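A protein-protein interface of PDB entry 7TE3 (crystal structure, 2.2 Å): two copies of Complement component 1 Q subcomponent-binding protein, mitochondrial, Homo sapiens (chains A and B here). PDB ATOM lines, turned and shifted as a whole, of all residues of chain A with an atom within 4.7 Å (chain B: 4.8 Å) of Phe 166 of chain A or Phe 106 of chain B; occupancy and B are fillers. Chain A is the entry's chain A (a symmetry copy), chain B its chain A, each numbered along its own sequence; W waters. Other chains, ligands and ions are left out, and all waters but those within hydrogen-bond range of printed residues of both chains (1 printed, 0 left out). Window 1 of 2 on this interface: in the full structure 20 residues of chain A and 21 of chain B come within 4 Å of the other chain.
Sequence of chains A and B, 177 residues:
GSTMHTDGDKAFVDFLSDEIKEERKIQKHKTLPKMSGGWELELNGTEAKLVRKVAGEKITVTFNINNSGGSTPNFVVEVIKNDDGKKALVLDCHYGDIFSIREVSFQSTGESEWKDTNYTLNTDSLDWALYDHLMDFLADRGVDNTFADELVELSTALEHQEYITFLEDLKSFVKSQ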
ATOM      1  N   GLU A 162      19.247 -28.660  -5.729  1.00  0.00           N
ATOM      2  CA  GLU A 162      18.171 -28.165  -6.584  1.00  0.00           C
ATOM      3  C   GLU A 162      18.134 -26.638  -6.625  1.00  0.00           C
ATOM      4  O   GLU A 162      17.819 -26.048  -7.666  1.00  0.00           O
ATOM      5  CB  GLU A 162      16.834 -28.720  -6.102  1.00  0.00           C
ATOM      6  CG  GLU A 162      16.651 -30.176  -6.405  1.00  0.00           C
ATOM      7  CD  GLU A 162      16.619 -30.420  -7.894  1.00  0.00           C
ATOM      8  OE1 GLU A 162      15.907 -29.676  -8.604  1.00  0.00           O
ATOM      9  OE2 GLU A 162      17.334 -31.330  -8.353  1.00  0.00           O
ATOM     10  N   TYR A 163      18.443 -25.980  -5.502  1.00  0.00           N
ATOM     11  CA  TYR A 163      18.530 -24.520  -5.497  1.00  0.00           C
ATOM     12  C   TYR A 163      19.633 -24.034  -6.430  1.00  0.00           C
ATOM     13  O   TYR A 163      19.431 -23.095  -7.210  1.00  0.00           O
ATOM     14  CB  TYR A 163      18.749 -24.014  -4.067  1.00  0.00           C
ATOM     15  CG  TYR A 163      19.079 -22.528  -3.972  1.00  0.00           C
ATOM     16  CD1 TYR A 163      18.108 -21.557  -4.238  1.00  0.00           C
ATOM     17  CD2 TYR A 163      20.356 -22.102  -3.614  1.00  0.00           C
ATOM     18  CE1 TYR A 163      18.404 -20.204  -4.163  1.00  0.00           C
ATOM     19  CE2 TYR A 163      20.669 -20.739  -3.527  1.00  0.00           C
ATOM     20  CZ  TYR A 163      19.684 -19.802  -3.802  1.00  0.00           C
ATOM     21  OH  TYR A 163      19.977 -18.469  -3.724  1.00  0.00           O
ATOM     22  N   ILE A 164      20.799 -24.678  -6.383  1.00  0.00           N
ATOM     23  CA  ILE A 164      21.886 -24.335  -7.300  1.00  0.00           C
ATOM     24  C   ILE A 164      21.450 -24.515  -8.747  1.00  0.00           C
ATOM     25  O   ILE A 164      21.748 -23.682  -9.613  1.00  0.00           O
ATOM     26  CB  ILE A 164      23.140 -25.175  -6.992  1.00  0.00           C
ATOM     27  CG1 ILE A 164      23.696 -24.851  -5.607  1.00  0.00           C
ATOM     28  CG2 ILE A 164      24.216 -24.931  -8.038  1.00  0.00           C
ATOM     29  CD1 ILE A 164      25.018 -25.517  -5.322  1.00  0.00           C
ATOM     30  N   THR A 165      20.740 -25.612  -9.036  1.00  0.00           N
ATOM     31  CA  THR A 165      20.236 -25.847 -10.386  1.00  0.00           C
ATOM     32  C   THR A 165      19.247 -24.764 -10.776  1.00  0.00           C
ATOM     33  O   THR A 165      19.218 -24.318 -11.929  1.00  0.00           O
ATOM     34  CB  THR A 165      19.596 -27.236 -10.461  1.00  0.00           C
ATOM     35  OG1 THR A 165      20.594 -28.219 -10.158  1.00  0.00           O
ATOM     36  CG2 THR A 165      19.008 -27.515 -11.833  1.00  0.00           C
ATOM     37  N   PHE A 166      18.452 -24.305  -9.807  1.00  0.00           N
ATOM     38  CA  PHE A 166      17.502 -23.228 -10.061  1.00  0.00           C
ATOM     39  C   PHE A 166      18.203 -21.908 -10.401  1.00  0.00           C
ATOM     40  O   PHE A 166      17.797 -21.211 -11.335  1.00  0.00           O
ATOM     41  CB  PHE A 166      16.586 -23.052  -8.854  1.00  0.00           C
ATOM     42  CG  PHE A 166      15.687 -21.875  -8.972  1.00  0.00           C
ATOM     43  CD1 PHE A 166      14.583 -21.924  -9.803  1.00  0.00           C
ATOM     44  CD2 PHE A 166      15.962 -20.712  -8.294  1.00  0.00           C
ATOM     45  CE1 PHE A 166      13.762 -20.832  -9.944  1.00  0.00           C
ATOM     46  CE2 PHE A 166      15.135 -19.611  -8.410  1.00  0.00           C
ATOM     47  CZ  PHE A 166      14.038 -19.666  -9.239  1.00  0.00           C
ATOM     48  N   LEU A 167      19.236 -21.532  -9.646  1.00  0.00           N
ATOM     49  CA  LEU A 167      20.003 -20.332  -9.989  1.00  0.00           C
ATOM     50  C   LEU A 167      20.596 -20.427 -11.391  1.00  0.00           C
ATOM     51  O   LEU A 167      20.609 -19.443 -12.144  1.00  0.00           O
ATOM     52  CB  LEU A 167      21.113 -20.118  -8.971  1.00  0.00           C
ATOM     53  CG  LEU A 167      20.664 -19.772  -7.558  1.00  0.00           C
ATOM     54  CD1 LEU A 167      21.904 -19.615  -6.663  1.00  0.00           C
ATOM     55  CD2 LEU A 167      19.786 -18.520  -7.568  1.00  0.00           C
ATOM     56  N   GLU A 168      21.111 -21.602 -11.755  1.00  0.00           N
ATOM     57  CA  GLU A 168      21.602 -21.787 -13.115  1.00  0.00           C
ATOM     58  C   GLU A 168      20.477 -21.624 -14.128  1.00  0.00           C
ATOM     59  O   GLU A 168      20.628 -20.903 -15.124  1.00  0.00           O
ATOM     60  CB  GLU A 168      22.281 -23.143 -13.232  1.00  0.00           C
ATOM     61  CG  GLU A 168      23.662 -23.098 -12.612  1.00  0.00           C
ATOM     62  CD  GLU A 168      24.262 -24.459 -12.370  1.00  0.00           C
ATOM     63  OE1 GLU A 168      23.503 -25.445 -12.236  1.00  0.00           O
ATOM     64  OE2 GLU A 168      25.507 -24.541 -12.305  1.00  0.00           O
ATOM     65  N   ASP A 169      19.317 -22.238 -13.865  1.00  0.00           N
ATOM     66  CA  ASP A 169      18.198 -22.087 -14.791  1.00  0.00           C
ATOM     67  C   ASP A 169      17.759 -20.632 -14.879  1.00  0.00           C
ATOM     68  O   ASP A 169      17.468 -20.120 -15.967  1.00  0.00           O
ATOM     69  CB  ASP A 169      17.034 -22.989 -14.372  1.00  0.00           C
ATOM     70  CG  ASP A 169      17.328 -24.458 -14.592  1.00  0.00           C
ATOM     71  OD1 ASP A 169      18.262 -24.762 -15.356  1.00  0.00           O
ATOM     72  OD2 ASP A 169      16.628 -25.309 -14.004  1.00  0.00           O
ATOM     73  N   LEU A 170      17.740 -19.936 -13.745  1.00  0.00           N
ATOM     74  CA  LEU A 170      17.372 -18.526 -13.755  1.00  0.00           C
ATOM     75  C   LEU A 170      18.397 -17.704 -14.525  1.00  0.00           C
ATOM     76  O   LEU A 170      18.036 -16.870 -15.363  1.00  0.00           O
ATOM     77  CB  LEU A 170      17.222 -18.035 -12.318  1.00  0.00           C
ATOM     78  CG  LEU A 170      16.780 -16.597 -12.077  1.00  0.00           C
ATOM     79  CD1 LEU A 170      15.431 -16.278 -12.743  1.00  0.00           C
ATOM     80  CD2 LEU A 170      16.711 -16.372 -10.581  1.00  0.00           C
ATOM     81  N   PHE A 173      17.928 -18.366 -18.114  1.00  0.00           N
ATOM     82  CA  PHE A 173      16.707 -17.725 -18.579  1.00  0.00           C
ATOM     83  C   PHE A 173      16.919 -16.236 -18.808  1.00  0.00           C
ATOM     84  O   PHE A 173      16.608 -15.708 -19.881  1.00  0.00           O
ATOM     85  CB  PHE A 173      15.588 -17.968 -17.564  1.00  0.00           C
ATOM     86  CG  PHE A 173      14.293 -17.341 -17.936  1.00  0.00           C
ATOM     87  CD1 PHE A 173      13.393 -18.013 -18.771  1.00  0.00           C
ATOM     88  CD2 PHE A 173      13.959 -16.092 -17.461  1.00  0.00           C
ATOM     89  CE1 PHE A 173      12.184 -17.431 -19.129  1.00  0.00           C
ATOM     90  CE2 PHE A 173      12.746 -15.504 -17.798  1.00  0.00           C
ATOM     91  CZ  PHE A 173      11.859 -16.174 -18.634  1.00  0.00           C
ATOM     92  N   LYS B  87       8.993 -23.484 -21.219  1.00  0.00           N
ATOM     93  CA  LYS B  87       9.215 -23.231 -19.798  1.00  0.00           C
ATOM     94  C   LYS B  87       9.068 -21.747 -19.507  1.00  0.00           C
ATOM     95  O   LYS B  87       9.727 -20.909 -20.128  1.00  0.00           O
ATOM     96  CB  LYS B  87      10.581 -23.736 -19.316  1.00  0.00           C
ATOM     97  CG  LYS B  87      11.782 -23.024 -19.883  1.00  0.00           C
ATOM     98  CD  LYS B  87      12.841 -22.802 -18.791  1.00  0.00           C
ATOM     99  CE  LYS B  87      13.173 -24.099 -18.068  1.00  0.00           C
ATOM    100  NZ  LYS B  87      14.551 -24.068 -17.495  1.00  0.00           N
ATOM    101  N   ALA B  88       8.214 -21.426 -18.553  1.00  0.00           N
ATOM    102  CA  ALA B  88       7.977 -20.046 -18.191  1.00  0.00           C
ATOM    103  C   ALA B  88       8.478 -19.810 -16.772  1.00  0.00           C
ATOM    104  O   ALA B  88       8.380 -20.695 -15.911  1.00  0.00           O
ATOM    105  CB  ALA B  88       6.491 -19.708 -18.320  1.00  0.00           C
ATOM    106  N   LEU B  89       9.024 -18.621 -16.534  1.00  0.00           N
ATOM    107  CA  LEU B  89       9.289 -18.162 -15.167  1.00  0.00           C
ATOM    108  C   LEU B  89       7.977 -17.700 -14.543  1.00  0.00           C
ATOM    109  O   LEU B  89       7.300 -16.829 -15.096  1.00  0.00           O
ATOM    110  CB  LEU B  89      10.308 -17.025 -15.177  1.00  0.00           C
ATOM    111  CG  LEU B  89      10.825 -16.572 -13.806  1.00  0.00           C
ATOM    112  CD1 LEU B  89      11.559 -17.711 -13.121  1.00  0.00           C
ATOM    113  CD2 LEU B  89      11.726 -15.371 -13.979  1.00  0.00           C
ATOM    114  N   VAL B 104       8.911 -18.245  -6.555  1.00  0.00           N
ATOM    115  CA  VAL B 104       9.335 -18.245  -7.950  1.00  0.00           C
ATOM    116  C   VAL B 104       9.659 -19.669  -8.374  1.00  0.00           C
ATOM    117  O   VAL B 104      10.296 -20.416  -7.617  1.00  0.00           O
ATOM    118  CB  VAL B 104      10.552 -17.325  -8.177  1.00  0.00           C
ATOM    119  CG1 VAL B 104      10.918 -17.287  -9.655  1.00  0.00           C
ATOM    120  CG2 VAL B 104      10.259 -15.921  -7.668  1.00  0.00           C
ATOM    121  N   SER B 105       9.231 -20.056  -9.584  1.00  0.00           N
ATOM    122  CA  SER B 105       9.635 -21.337 -10.154  1.00  0.00           C
ATOM    123  C   SER B 105       9.506 -21.293 -11.670  1.00  0.00           C
ATOM    124  O   SER B 105       8.940 -20.360 -12.246  1.00  0.00           O
ATOM    125  CB  SER B 105       8.816 -22.497  -9.602  1.00  0.00           C
ATOM    126  OG  SER B 105       7.498 -22.410 -10.064  1.00  0.00           O
ATOM    127  N   PHE B 106      10.052 -22.321 -12.312  1.00  0.00           N
ATOM    128  CA  PHE B 106       9.816 -22.563 -13.726  1.00  0.00           C
ATOM    129  C   PHE B 106       8.712 -23.592 -13.862  1.00  0.00           C
ATOM    130  O   PHE B 106       8.671 -24.580 -13.120  1.00  0.00           O
ATOM    131  CB  PHE B 106      11.071 -23.056 -14.448  1.00  0.00           C
ATOM    132  CG  PHE B 106      12.156 -22.026 -14.541  1.00  0.00           C
ATOM    133  CD1 PHE B 106      12.147 -21.084 -15.549  1.00  0.00           C
ATOM    134  CD2 PHE B 106      13.189 -22.004 -13.615  1.00  0.00           C
ATOM    135  CE1 PHE B 106      13.154 -20.133 -15.634  1.00  0.00           C
ATOM    136  CE2 PHE B 106      14.197 -21.048 -13.691  1.00  0.00           C
ATOM    137  CZ  PHE B 106      14.186 -20.119 -14.696  1.00  0.00           C
ATOM    138  N   GLN B 107       7.801 -23.336 -14.791  1.00  0.00           N
ATOM    139  CA  GLN B 107       6.696 -24.247 -15.038  1.00  0.00           C
ATOM    140  C   GLN B 107       6.533 -24.415 -16.534  1.00  0.00           C
ATOM    141  O   GLN B 107       6.911 -23.530 -17.309  1.00  0.00           O
ATOM    142  CB  GLN B 107       5.399 -23.723 -14.414  1.00  0.00           C
ATOM    143  CG  GLN B 107       5.474 -23.581 -12.902  1.00  0.00           C
ATOM    144  CD  GLN B 107       5.472 -24.918 -12.201  1.00  0.00           C
ATOM    145  OE1 GLN B 107       4.892 -25.872 -12.689  1.00  0.00           O
ATOM    146  NE2 GLN B 107       6.132 -24.994 -11.052  1.00  0.00           N
ATOM    147  N   SER B 108       5.983 -25.558 -16.942  1.00  0.00           N
ATOM    148  CA  SER B 108       5.583 -25.696 -18.334  1.00  0.00           C
ATOM    149  C   SER B 108       4.373 -24.808 -18.590  1.00  0.00           C
ATOM    150  O   SER B 108       3.444 -24.738 -17.777  1.00  0.00           O
ATOM    151  CB  SER B 108       5.262 -27.152 -18.690  1.00  0.00           C
ATOM    152  OG  SER B 108       6.214 -28.054 -18.147  1.00  0.00           O
ATOM    153  N   ASN B 118       9.127 -29.380  -9.750  1.00  0.00           N
ATOM    154  CA  ASN B 118      10.013 -28.300 -10.138  1.00  0.00           C
ATOM    155  C   ASN B 118      10.332 -27.465  -8.912  1.00  0.00           C
ATOM    156  O   ASN B 118       9.492 -27.286  -8.029  1.00  0.00           O
ATOM    157  CB  ASN B 118       9.389 -27.433 -11.224  1.00  0.00           C
ATOM    158  CG  ASN B 118       9.387 -28.124 -12.580  1.00  0.00           C
ATOM    159  OD1 ASN B 118      10.019 -29.161 -12.752  1.00  0.00           O
ATOM    160  ND2 ASN B 118       8.686 -27.547 -13.540  1.00  0.00           N
ATOM    161  N   TYR B 119      11.561 -26.968  -8.862  1.00  0.00           N
ATOM    162  CA  TYR B 119      12.025 -26.266  -7.681  1.00  0.00           C
ATOM    163  C   TYR B 119      11.257 -24.964  -7.507  1.00  0.00           C
ATOM    164  O   TYR B 119      11.050 -24.212  -8.460  1.00  0.00           O
ATOM    165  CB  TYR B 119      13.526 -25.990  -7.777  1.00  0.00           C
ATOM    166  CG  TYR B 119      14.041 -25.279  -6.553  1.00  0.00           C
ATOM    167  CD1 TYR B 119      14.396 -25.994  -5.428  1.00  0.00           C
ATOM    168  CD2 TYR B 119      14.134 -23.893  -6.510  1.00  0.00           C
ATOM    169  CE1 TYR B 119      14.836 -25.372  -4.309  1.00  0.00           C
ATOM    170  CE2 TYR B 119      14.585 -23.252  -5.384  1.00  0.00           C
ATOM    171  CZ  TYR B 119      14.931 -24.003  -4.282  1.00  0.00           C
ATOM    172  OH  TYR B 119      15.378 -23.401  -3.133  1.00  0.00           O
ATOM    173  N   LEU B 121      11.333 -21.443  -5.396  1.00  0.00           N
ATOM    174  CA  LEU B 121      12.021 -20.502  -4.524  1.00  0.00           C
ATOM    175  C   LEU B 121      10.974 -19.807  -3.659  1.00  0.00           C
ATOM    176  O   LEU B 121      10.273 -18.900  -4.118  1.00  0.00           O
ATOM    177  CB  LEU B 121      12.824 -19.491  -5.335  1.00  0.00           C
ATOM    178  CG  LEU B 121      13.672 -18.508  -4.497  1.00  0.00           C
ATOM    179  CD1 LEU B 121      14.729 -19.243  -3.701  1.00  0.00           C
ATOM    180  CD2 LEU B 121      14.345 -17.464  -5.373  1.00  0.00           C
HETATM  181  O   HOH W   1      16.372 -21.821 -18.023  1.00  0.00           O
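No position is printed for both chains.
Of the 11 pairs that touch across the chains among the printed residues, none has its exchanged pair printed and touching as well.
Water W1 lies within hydrogen-bond range of the backbone carbonyl oxygen of Asp 169 of chain A and the side-chain amino group of Lys 87 of chain B.
The backbone carbonyl oxygen (O) of Val 104 of chain B sits at hydrogen-bond distance from the backbone NH (N) of Leu 121 of chain B (2.7 Å).
The backbone carbonyl oxygen (O) of Phe 106 of chain B lies within hydrogen-bond range of the side-chain amide nitrogen (ND2) of Asn 118 of chain B.
Tyr 119 of chain B touches Glu 162 of chain A.
Tyr 119 of chain B touches Tyr 163 of chain A (OH to CD1, 3.5 Å).
CD1 of Leu 121 of chain B touches CE1 of Tyr 163 of chain A, at 3.8 Å.
Val 104 of chain B touches Phe 166 of chain A (CG1 to CZ, 3.9 Å).
CE1 of Phe 166 of chain A touches CE2 of Phe 106 of chain B, 3.8 Å away.
Phe 166 of chain A touches Tyr 119 of chain B.
Phe 166 of chain A touches Leu 121 of chain B (CE2 to CD2, 3.8 Å).
CZ of Phe 106 of chain B touches N of Leu 170 of chain A, at 3.7 Å.
Phe 173 of chain A touches Leu 89 of chain B (CZ to CB, 3.9 Å).
CB of Phe 173 of chain A touches CE1 of Phe 106 of chain B (3.8 Å).
Of chain B, only Val 104 (3.9 Å), Phe 106 (3.8 Å), Tyr 119 (3.5 Å) and Leu 121 (3.8 Å) come within 4 Å of Phe 166 of chain A.
Phe 106 of chain B touches just these residues of chain A: Phe 166 (3.8 Å), Asp 169 (3.5 Å), Leu 170 (3.7 Å) and Phe 173 (3.8 Å).
Printed residues of chain B within 4 Å of Tyr 163 of chain A: Tyr 119 and Leu 121.
Of the printed residues of chain B, Phe 173 of chain A touches Leu 89 and Phe 106.
The nearest residue of chain B that does not touch Phe 166 of chain A is Ser 105 of chain B (4.2 Å).
The nearest printed residue of chain A that does not touch Phe 106 of chain B is Thr 165 of chain A (6.2 Å).
Of the 11 printed residues of chain B, 5 touch a printed residue of chain A.
Hydrophobic or aromatic side chains of chain B that line the printed part of chain A: Leu 89, Val 104, Phe 106, Tyr 119 and Leu 121.
Among the printed residues, no Asp or Glu carboxylate lies within 4 Å of a Lys or Arg side-chain nitrogen of the other chain.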
